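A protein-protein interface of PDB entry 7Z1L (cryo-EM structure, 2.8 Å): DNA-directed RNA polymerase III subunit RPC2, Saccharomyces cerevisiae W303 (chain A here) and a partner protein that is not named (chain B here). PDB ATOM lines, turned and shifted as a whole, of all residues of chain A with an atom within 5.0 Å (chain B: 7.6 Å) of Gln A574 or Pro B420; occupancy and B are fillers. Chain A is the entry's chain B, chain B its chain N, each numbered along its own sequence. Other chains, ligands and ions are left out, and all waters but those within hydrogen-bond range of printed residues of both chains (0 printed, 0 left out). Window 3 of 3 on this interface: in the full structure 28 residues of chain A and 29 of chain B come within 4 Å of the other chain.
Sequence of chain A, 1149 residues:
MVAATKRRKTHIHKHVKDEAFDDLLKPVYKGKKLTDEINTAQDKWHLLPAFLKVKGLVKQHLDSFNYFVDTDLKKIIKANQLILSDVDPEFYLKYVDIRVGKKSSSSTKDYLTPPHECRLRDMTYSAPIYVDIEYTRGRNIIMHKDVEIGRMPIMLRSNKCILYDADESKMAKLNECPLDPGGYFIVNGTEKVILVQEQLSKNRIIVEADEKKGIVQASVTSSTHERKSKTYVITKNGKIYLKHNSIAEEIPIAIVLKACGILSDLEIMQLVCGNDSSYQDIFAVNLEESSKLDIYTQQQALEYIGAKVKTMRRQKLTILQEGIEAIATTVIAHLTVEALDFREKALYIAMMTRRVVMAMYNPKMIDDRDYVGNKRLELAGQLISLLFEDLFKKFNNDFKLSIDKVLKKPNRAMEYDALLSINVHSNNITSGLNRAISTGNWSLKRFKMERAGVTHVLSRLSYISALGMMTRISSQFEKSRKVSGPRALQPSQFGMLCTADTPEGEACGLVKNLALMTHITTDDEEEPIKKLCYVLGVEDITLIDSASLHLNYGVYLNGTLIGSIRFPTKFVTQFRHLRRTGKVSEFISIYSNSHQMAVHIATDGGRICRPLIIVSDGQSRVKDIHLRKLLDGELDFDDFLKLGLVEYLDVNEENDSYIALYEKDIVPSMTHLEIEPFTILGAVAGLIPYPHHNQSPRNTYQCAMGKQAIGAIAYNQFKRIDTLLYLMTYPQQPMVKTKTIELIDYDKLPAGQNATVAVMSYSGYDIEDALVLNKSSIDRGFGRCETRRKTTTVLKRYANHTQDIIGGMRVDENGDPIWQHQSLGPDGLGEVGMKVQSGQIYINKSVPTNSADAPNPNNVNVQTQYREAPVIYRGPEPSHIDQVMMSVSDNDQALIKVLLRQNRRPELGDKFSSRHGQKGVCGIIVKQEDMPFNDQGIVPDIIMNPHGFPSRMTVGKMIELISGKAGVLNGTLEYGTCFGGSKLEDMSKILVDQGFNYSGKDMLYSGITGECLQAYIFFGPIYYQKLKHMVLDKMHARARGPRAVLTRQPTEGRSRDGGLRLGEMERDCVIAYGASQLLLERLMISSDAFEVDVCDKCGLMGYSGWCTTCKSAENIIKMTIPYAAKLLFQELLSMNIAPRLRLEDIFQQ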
ATOM      1  N   VAL A 535      11.092 -31.987   4.156  1.00  0.00           N
ATOM      2  CA  VAL A 535      11.374 -31.350   2.871  1.00  0.00           C
ATOM      3  C   VAL A 535      10.962 -29.881   2.888  1.00  0.00           C
ATOM      4  O   VAL A 535      11.700 -29.013   2.406  1.00  0.00           O
ATOM      5  CB  VAL A 535      10.684 -32.124   1.732  1.00  0.00           C
ATOM      6  CG1 VAL A 535      10.696 -31.313   0.452  1.00  0.00           C
ATOM      7  CG2 VAL A 535      11.377 -33.456   1.507  1.00  0.00           C
ATOM      8  N   LEU A 536       9.798 -29.572   3.465  1.00  0.00           N
ATOM      9  CA  LEU A 536       9.246 -28.222   3.391  1.00  0.00           C
ATOM     10  C   LEU A 536      10.036 -27.195   4.193  1.00  0.00           C
ATOM     11  O   LEU A 536       9.758 -25.998   4.063  1.00  0.00           O
ATOM     12  CB  LEU A 536       7.789 -28.217   3.857  1.00  0.00           C
ATOM     13  CG  LEU A 536       6.749 -28.692   2.841  1.00  0.00           C
ATOM     14  CD1 LEU A 536       5.361 -28.659   3.443  1.00  0.00           C
ATOM     15  CD2 LEU A 536       6.805 -27.847   1.582  1.00  0.00           C
ATOM     16  N   THR A 569       3.835 -19.397   9.247  1.00  0.00           N
ATOM     17  CA  THR A 569       2.688 -19.073   8.401  1.00  0.00           C
ATOM     18  C   THR A 569       2.889 -19.571   6.973  1.00  0.00           C
ATOM     19  O   THR A 569       1.954 -20.099   6.359  1.00  0.00           O
ATOM     20  CB  THR A 569       2.427 -17.568   8.415  1.00  0.00           C
ATOM     21  OG1 THR A 569       2.308 -17.116   9.768  1.00  0.00           O
ATOM     22  CG2 THR A 569       1.145 -17.239   7.670  1.00  0.00           C
ATOM     23  N   LYS A 570       4.101 -19.422   6.433  1.00  0.00           N
ATOM     24  CA  LYS A 570       4.378 -19.929   5.093  1.00  0.00           C
ATOM     25  C   LYS A 570       4.300 -21.450   5.051  1.00  0.00           C
ATOM     26  O   LYS A 570       3.794 -22.024   4.080  1.00  0.00           O
ATOM     27  CB  LYS A 570       5.748 -19.450   4.619  1.00  0.00           C
ATOM     28  CG  LYS A 570       6.002 -19.688   3.142  1.00  0.00           C
ATOM     29  CD  LYS A 570       7.477 -19.566   2.809  1.00  0.00           C
ATOM     30  CE  LYS A 570       7.980 -18.156   3.063  1.00  0.00           C
ATOM     31  NZ  LYS A 570       9.438 -18.138   3.359  1.00  0.00           N
ATOM     32  N   PHE A 571       4.792 -22.117   6.098  1.00  0.00           N
ATOM     33  CA  PHE A 571       4.701 -23.571   6.176  1.00  0.00           C
ATOM     34  C   PHE A 571       3.249 -24.033   6.217  1.00  0.00           C
ATOM     35  O   PHE A 571       2.871 -24.988   5.526  1.00  0.00           O
ATOM     36  CB  PHE A 571       5.462 -24.063   7.406  1.00  0.00           C
ATOM     37  CG  PHE A 571       5.385 -25.545   7.626  1.00  0.00           C
ATOM     38  CD1 PHE A 571       6.196 -26.406   6.914  1.00  0.00           C
ATOM     39  CD2 PHE A 571       4.520 -26.075   8.569  1.00  0.00           C
ATOM     40  CE1 PHE A 571       6.134 -27.767   7.122  1.00  0.00           C
ATOM     41  CE2 PHE A 571       4.453 -27.435   8.780  1.00  0.00           C
ATOM     42  CZ  PHE A 571       5.262 -28.281   8.057  1.00  0.00           C
ATOM     43  N   VAL A 572       2.419 -23.351   7.011  1.00  0.00           N
ATOM     44  CA  VAL A 572       1.004 -23.703   7.111  1.00  0.00           C
ATOM     45  C   VAL A 572       0.296 -23.470   5.781  1.00  0.00           C
ATOM     46  O   VAL A 572      -0.505 -24.302   5.335  1.00  0.00           O
ATOM     47  CB  VAL A 572       0.349 -22.914   8.260  1.00  0.00           C
ATOM     48  CG1 VAL A 572      -1.160 -22.958   8.159  1.00  0.00           C
ATOM     49  CG2 VAL A 572       0.799 -23.468   9.598  1.00  0.00           C
ATOM     50  N   THR A 573       0.590 -22.345   5.122  1.00  0.00           N
ATOM     51  CA  THR A 573      -0.022 -22.051   3.829  1.00  0.00           C
ATOM     52  C   THR A 573       0.383 -23.077   2.775  1.00  0.00           C
ATOM     53  O   THR A 573      -0.457 -23.543   1.996  1.00  0.00           O
ATOM     54  CB  THR A 573       0.357 -20.636   3.385  1.00  0.00           C
ATOM     55  OG1 THR A 573      -0.305 -19.681   4.222  1.00  0.00           O
ATOM     56  CG2 THR A 573      -0.047 -20.386   1.941  1.00  0.00           C
ATOM     57  N   GLN A 574       1.663 -23.458   2.752  1.00  0.00           N
ATOM     58  CA  GLN A 574       2.128 -24.459   1.798  1.00  0.00           C
ATOM     59  C   GLN A 574       1.492 -25.818   2.058  1.00  0.00           C
ATOM     60  O   GLN A 574       1.120 -26.530   1.115  1.00  0.00           O
ATOM     61  CB  GLN A 574       3.651 -24.557   1.854  1.00  0.00           C
ATOM     62  CG  GLN A 574       4.365 -23.410   1.164  1.00  0.00           C
ATOM     63  CD  GLN A 574       5.866 -23.600   1.121  1.00  0.00           C
ATOM     64  OE1 GLN A 574       6.399 -24.538   1.711  1.00  0.00           O
ATOM     65  NE2 GLN A 574       6.556 -22.710   0.420  1.00  0.00           N
ATOM     66  N   PHE A 575       1.353 -26.198   3.330  1.00  0.00           N
ATOM     67  CA  PHE A 575       0.716 -27.471   3.651  1.00  0.00           C
ATOM     68  C   PHE A 575      -0.761 -27.464   3.272  1.00  0.00           C
ATOM     69  O   PHE A 575      -1.283 -28.467   2.770  1.00  0.00           O
ATOM     70  CB  PHE A 575       0.895 -27.785   5.134  1.00  0.00           C
ATOM     71  CG  PHE A 575       0.962 -29.250   5.435  1.00  0.00           C
ATOM     72  CD1 PHE A 575      -0.192 -29.973   5.678  1.00  0.00           C
ATOM     73  CD2 PHE A 575       2.178 -29.906   5.475  1.00  0.00           C
ATOM     74  CE1 PHE A 575      -0.132 -31.323   5.955  1.00  0.00           C
ATOM     75  CE2 PHE A 575       2.245 -31.253   5.751  1.00  0.00           C
ATOM     76  CZ  PHE A 575       1.089 -31.963   5.992  1.00  0.00           C
ATOM     77  N   ARG A 576      -1.450 -26.340   3.492  1.00  0.00           N
ATOM     78  CA  ARG A 576      -2.841 -26.233   3.065  1.00  0.00           C
ATOM     79  C   ARG A 576      -2.962 -26.300   1.549  1.00  0.00           C
ATOM     80  O   ARG A 576      -3.911 -26.890   1.023  1.00  0.00           O
ATOM     81  CB  ARG A 576      -3.471 -24.941   3.582  1.00  0.00           C
ATOM     82  CG  ARG A 576      -3.747 -24.915   5.070  1.00  0.00           C
ATOM     83  CD  ARG A 576      -4.553 -23.685   5.449  1.00  0.00           C
ATOM     84  NE  ARG A 576      -4.227 -23.196   6.782  1.00  0.00           N
ATOM     85  CZ  ARG A 576      -4.770 -23.654   7.901  1.00  0.00           C
ATOM     86  NH1 ARG A 576      -5.662 -24.629   7.886  1.00  0.00           N
ATOM     87  NH2 ARG A 576      -4.410 -23.120   9.064  1.00  0.00           N
ATOM     88  N   HIS A 577      -2.018 -25.687   0.829  1.00  0.00           N
ATOM     89  CA  HIS A 577      -2.039 -25.757  -0.628  1.00  0.00           C
ATOM     90  C   HIS A 577      -1.824 -27.184  -1.114  1.00  0.00           C
ATOM     91  O   HIS A 577      -2.464 -27.624  -2.075  1.00  0.00           O
ATOM     92  CB  HIS A 577      -0.981 -24.823  -1.215  1.00  0.00           C
ATOM     93  CG  HIS A 577      -0.891 -24.872  -2.707  1.00  0.00           C
ATOM     94  ND1 HIS A 577      -1.592 -24.010  -3.522  1.00  0.00           N
ATOM     95  CD2 HIS A 577      -0.178 -25.673  -3.533  1.00  0.00           C
ATOM     96  CE1 HIS A 577      -1.319 -24.280  -4.785  1.00  0.00           C
ATOM     97  NE2 HIS A 577      -0.463 -25.286  -4.820  1.00  0.00           N
ATOM     98  N   LEU A 578      -0.922 -27.921  -0.460  1.00  0.00           N
ATOM     99  CA  LEU A 578      -0.714 -29.321  -0.818  1.00  0.00           C
ATOM    100  C   LEU A 578      -1.951 -30.158  -0.520  1.00  0.00           C
ATOM    101  O   LEU A 578      -2.283 -31.078  -1.276  1.00  0.00           O
ATOM    102  CB  LEU A 578       0.499 -29.880  -0.079  1.00  0.00           C
ATOM    103  CG  LEU A 578       1.847 -29.489  -0.674  1.00  0.00           C
ATOM    104  CD1 LEU A 578       2.970 -30.219   0.024  1.00  0.00           C
ATOM    105  CD2 LEU A 578       1.865 -29.771  -2.164  1.00  0.00           C
ATOM    106  N   LEU B 309      19.065 -29.192   2.054  1.00  0.00           N
ATOM    107  CA  LEU B 309      18.319 -29.457   0.835  1.00  0.00           C
ATOM    108  C   LEU B 309      17.305 -30.570   1.060  1.00  0.00           C
ATOM    109  O   LEU B 309      17.443 -31.366   1.993  1.00  0.00           O
ATOM    110  CB  LEU B 309      19.273 -29.843  -0.305  1.00  0.00           C
ATOM    111  CG  LEU B 309      19.965 -28.726  -1.094  1.00  0.00           C
ATOM    112  CD1 LEU B 309      21.044 -28.040  -0.290  1.00  0.00           C
ATOM    113  CD2 LEU B 309      20.544 -29.275  -2.384  1.00  0.00           C
ATOM    114  N   PRO B 310      16.250 -30.634   0.243  1.00  0.00           N
ATOM    115  CA  PRO B 310      15.297 -31.746   0.358  1.00  0.00           C
ATOM    116  C   PRO B 310      15.967 -33.088   0.101  1.00  0.00           C
ATOM    117  O   PRO B 310      16.896 -33.197  -0.702  1.00  0.00           O
ATOM    118  CB  PRO B 310      14.244 -31.428  -0.709  1.00  0.00           C
ATOM    119  CG  PRO B 310      14.865 -30.395  -1.589  1.00  0.00           C
ATOM    120  CD  PRO B 310      15.781 -29.618  -0.714  1.00  0.00           C
ATOM    121  N   ARG B 312      15.069 -35.670  -1.433  1.00  0.00           N
ATOM    122  CA  ARG B 312      14.932 -36.196  -2.789  1.00  0.00           C
ATOM    123  C   ARG B 312      15.137 -35.042  -3.762  1.00  0.00           C
ATOM    124  O   ARG B 312      14.207 -34.277  -4.037  1.00  0.00           O
ATOM    125  CB  ARG B 312      13.578 -36.864  -3.001  1.00  0.00           C
ATOM    126  CG  ARG B 312      13.428 -37.494  -4.379  1.00  0.00           C
ATOM    127  CD  ARG B 312      12.093 -38.196  -4.540  1.00  0.00           C
ATOM    128  NE  ARG B 312      11.964 -38.833  -5.844  1.00  0.00           N
ATOM    129  CZ  ARG B 312      11.472 -38.238  -6.922  1.00  0.00           C
ATOM    130  NH1 ARG B 312      11.058 -36.983  -6.891  1.00  0.00           N
ATOM    131  NH2 ARG B 312      11.393 -38.921  -8.061  1.00  0.00           N
ATOM    132  N   VAL B 378      13.724 -26.540 -11.383  1.00  0.00           N
ATOM    133  CA  VAL B 378      12.807 -26.083 -10.344  1.00  0.00           C
ATOM    134  C   VAL B 378      13.498 -25.023  -9.495  1.00  0.00           C
ATOM    135  O   VAL B 378      14.663 -25.180  -9.104  1.00  0.00           O
ATOM    136  CB  VAL B 378      12.278 -27.256  -9.492  1.00  0.00           C
ATOM    137  CG1 VAL B 378      13.399 -28.030  -8.828  1.00  0.00           C
ATOM    138  CG2 VAL B 378      11.278 -26.760  -8.453  1.00  0.00           C
ATOM    139  N   VAL B 379      12.788 -23.922  -9.251  1.00  0.00           N
ATOM    140  CA  VAL B 379      13.256 -22.841  -8.393  1.00  0.00           C
ATOM    141  C   VAL B 379      12.745 -23.085  -6.981  1.00  0.00           C
ATOM    142  O   VAL B 379      11.640 -23.597  -6.773  1.00  0.00           O
ATOM    143  CB  VAL B 379      12.808 -21.467  -8.935  1.00  0.00           C
ATOM    144  CG1 VAL B 379      13.482 -21.181 -10.263  1.00  0.00           C
ATOM    145  CG2 VAL B 379      11.297 -21.413  -9.091  1.00  0.00           C
ATOM    146  N   MET B 380      13.569 -22.737  -5.996  1.00  0.00           N
ATOM    147  CA  MET B 380      13.263 -22.987  -4.599  1.00  0.00           C
ATOM    148  C   MET B 380      13.716 -21.798  -3.767  1.00  0.00           C
ATOM    149  O   MET B 380      14.593 -21.031  -4.178  1.00  0.00           O
ATOM    150  CB  MET B 380      13.942 -24.269  -4.096  1.00  0.00           C
ATOM    151  CG  MET B 380      13.429 -25.552  -4.731  1.00  0.00           C
ATOM    152  SD  MET B 380      14.205 -27.035  -4.065  1.00  0.00           S
ATOM    153  CE  MET B 380      15.818 -26.937  -4.820  1.00  0.00           C
ATOM    154  N   ASP B 381      13.113 -21.653  -2.590  1.00  0.00           N
ATOM    155  CA  ASP B 381      13.437 -20.553  -1.698  1.00  0.00           C
ATOM    156  C   ASP B 381      14.674 -20.883  -0.869  1.00  0.00           C
ATOM    157  O   ASP B 381      15.307 -21.930  -1.026  1.00  0.00           O
ATOM    158  CB  ASP B 381      12.248 -20.230  -0.799  1.00  0.00           C
ATOM    159  CG  ASP B 381      11.031 -19.797  -1.581  1.00  0.00           C
ATOM    160  OD1 ASP B 381      11.199 -19.378  -2.745  1.00  0.00           O
ATOM    161  OD2 ASP B 381       9.912 -19.872  -1.033  1.00  0.00           O
ATOM    162  N   ILE B 382      15.017 -19.971   0.035  1.00  0.00           N
ATOM    163  CA  ILE B 382      16.224 -20.086   0.846  1.00  0.00           C
ATOM    164  C   ILE B 382      16.037 -19.245   2.104  1.00  0.00           C
ATOM    165  O   ILE B 382      15.539 -18.117   2.040  1.00  0.00           O
ATOM    166  CB  ILE B 382      17.472 -19.661   0.043  1.00  0.00           C
ATOM    167  CG1 ILE B 382      18.738 -19.727   0.896  1.00  0.00           C
ATOM    168  CG2 ILE B 382      17.287 -18.288  -0.586  1.00  0.00           C
ATOM    169  CD1 ILE B 382      20.001 -19.579   0.086  1.00  0.00           C
ATOM    170  N   VAL B 418      16.742 -24.885   2.137  1.00  0.00           N
ATOM    171  CA  VAL B 418      16.152 -24.728   0.814  1.00  0.00           C
ATOM    172  C   VAL B 418      14.829 -25.481   0.793  1.00  0.00           C
ATOM    173  O   VAL B 418      14.785 -26.678   1.102  1.00  0.00           O
ATOM    174  CB  VAL B 418      17.102 -25.245  -0.280  1.00  0.00           C
ATOM    175  CG1 VAL B 418      16.526 -24.981  -1.652  1.00  0.00           C
ATOM    176  CG2 VAL B 418      18.470 -24.604  -0.137  1.00  0.00           C
ATOM    177  N   THR B 419      13.753 -24.784   0.430  1.00  0.00           N
ATOM    178  CA  THR B 419      12.426 -25.378   0.409  1.00  0.00           C
ATOM    179  C   THR B 419      11.776 -25.168  -0.952  1.00  0.00           C
ATOM    180  O   THR B 419      11.982 -24.127  -1.587  1.00  0.00           O
ATOM    181  CB  THR B 419      11.539 -24.782   1.521  1.00  0.00           C
ATOM    182  OG1 THR B 419      10.211 -25.311   1.424  1.00  0.00           O
ATOM    183  CG2 THR B 419      11.491 -23.260   1.442  1.00  0.00           C
ATOM    184  N   PRO B 420      11.003 -26.145  -1.436  1.00  0.00           N
ATOM    185  CA  PRO B 420      10.382 -26.010  -2.760  1.00  0.00           C
ATOM    186  C   PRO B 420       9.401 -24.849  -2.830  1.00  0.00           C
ATOM    187  O   PRO B 420       8.700 -24.534  -1.866  1.00  0.00           O
ATOM    188  CB  PRO B 420       9.669 -27.351  -2.957  1.00  0.00           C
ATOM    189  CG  PRO B 420      10.377 -28.297  -2.062  1.00  0.00           C
ATOM    190  CD  PRO B 420      10.831 -27.498  -0.882  1.00  0.00           C
ATOM    191  N   GLN B 421       9.360 -24.212  -3.998  1.00  0.00           N
ATOM    192  CA  GLN B 421       8.444 -23.109  -4.265  1.00  0.00           C
ATOM    193  C   GLN B 421       7.120 -23.682  -4.752  1.00  0.00           C
ATOM    194  O   GLN B 421       6.985 -24.049  -5.924  1.00  0.00           O
ATOM    195  CB  GLN B 421       9.041 -22.147  -5.290  1.00  0.00           C
ATOM    196  CG  GLN B 421       8.121 -21.002  -5.715  1.00  0.00           C
ATOM    197  CD  GLN B 421       7.928 -19.942  -4.644  1.00  0.00           C
ATOM    198  OE1 GLN B 421       8.559 -19.977  -3.590  1.00  0.00           O
ATOM    199  NE2 GLN B 421       7.044 -18.989  -4.916  1.00  0.00           N
ATOM    200  N   ILE B 422       6.147 -23.775  -3.850  1.00  0.00           N
ATOM    201  CA  ILE B 422       4.843 -24.328  -4.185  1.00  0.00           C
ATOM    202  C   ILE B 422       3.751 -23.303  -3.910  1.00  0.00           C
ATOM    203  O   ILE B 422       4.001 -22.269  -3.291  1.00  0.00           O
ATOM    204  CB  ILE B 422       4.573 -25.630  -3.414  1.00  0.00           C
ATOM    205  CG1 ILE B 422       4.232 -25.329  -1.959  1.00  0.00           C
ATOM    206  CG2 ILE B 422       5.779 -26.539  -3.459  1.00  0.00           C
ATOM    207  CD1 ILE B 422       4.012 -26.568  -1.134  1.00  0.00           C
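The backbone NH (N) of Asp B381 is in hydrogen-bond range of the backbone carbonyl oxygen (O) of Thr B419, at 2.9 Å.
Among the printed residues, merely in contact across the chains: Gln A574 with Ile B422 (3.6 Å), Gln A574 with Pro B420 (3.6 Å), Leu A578 with Ile B422 (3.7 Å), Val A535 with Pro B420 (3.7 Å), Val A535 with Pro B310 (3.7 Å) and Gln A574 with Thr B419 (3.9 Å).
Of the 12 printed residues of chain A, 4 touch a printed residue of chain B. Hydrophobic or aromatic side chains of chain A that line the printed part of chain B: Val A535 and Leu A578. Hydrophobic or aromatic side chains of chain B that line the printed part of chain A: Pro B310, Pro B420 and Ile B422. Along chain B the printed residues that touch a printed residue of chain A span positions 310 to 422. Among the printed residues, 7 pairs touch across the chains. Among the printed residues, no Asp or Glu carboxylate lies within 4 Å of a Lys or Arg side-chain nitrogen of the other chain.
O of Leu A536 is in hydrogen-bond range of OG1 of Thr B419 (2.8 Å).
Gln A574 touches three residues of chain B. Pro B420 touches just these residues of chain A: Val A535 (3.7 Å) and Gln A574 (3.6 Å). Of the printed residues of chain B, Leu A578 touches Ile B422 (3.7 Å). Printed residues of chain B within 4 Å of Leu A536: Thr B419. Val A572 touches none of the printed residues of chain B. Val B378 touches none of the printed residues of chain A. The nearest residue of chain A that does not touch Pro B420 is Leu A536 (4.6 Å). The nearest printed residue of chain B that does not touch Val A535 is Val B418 (4.1 Å).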
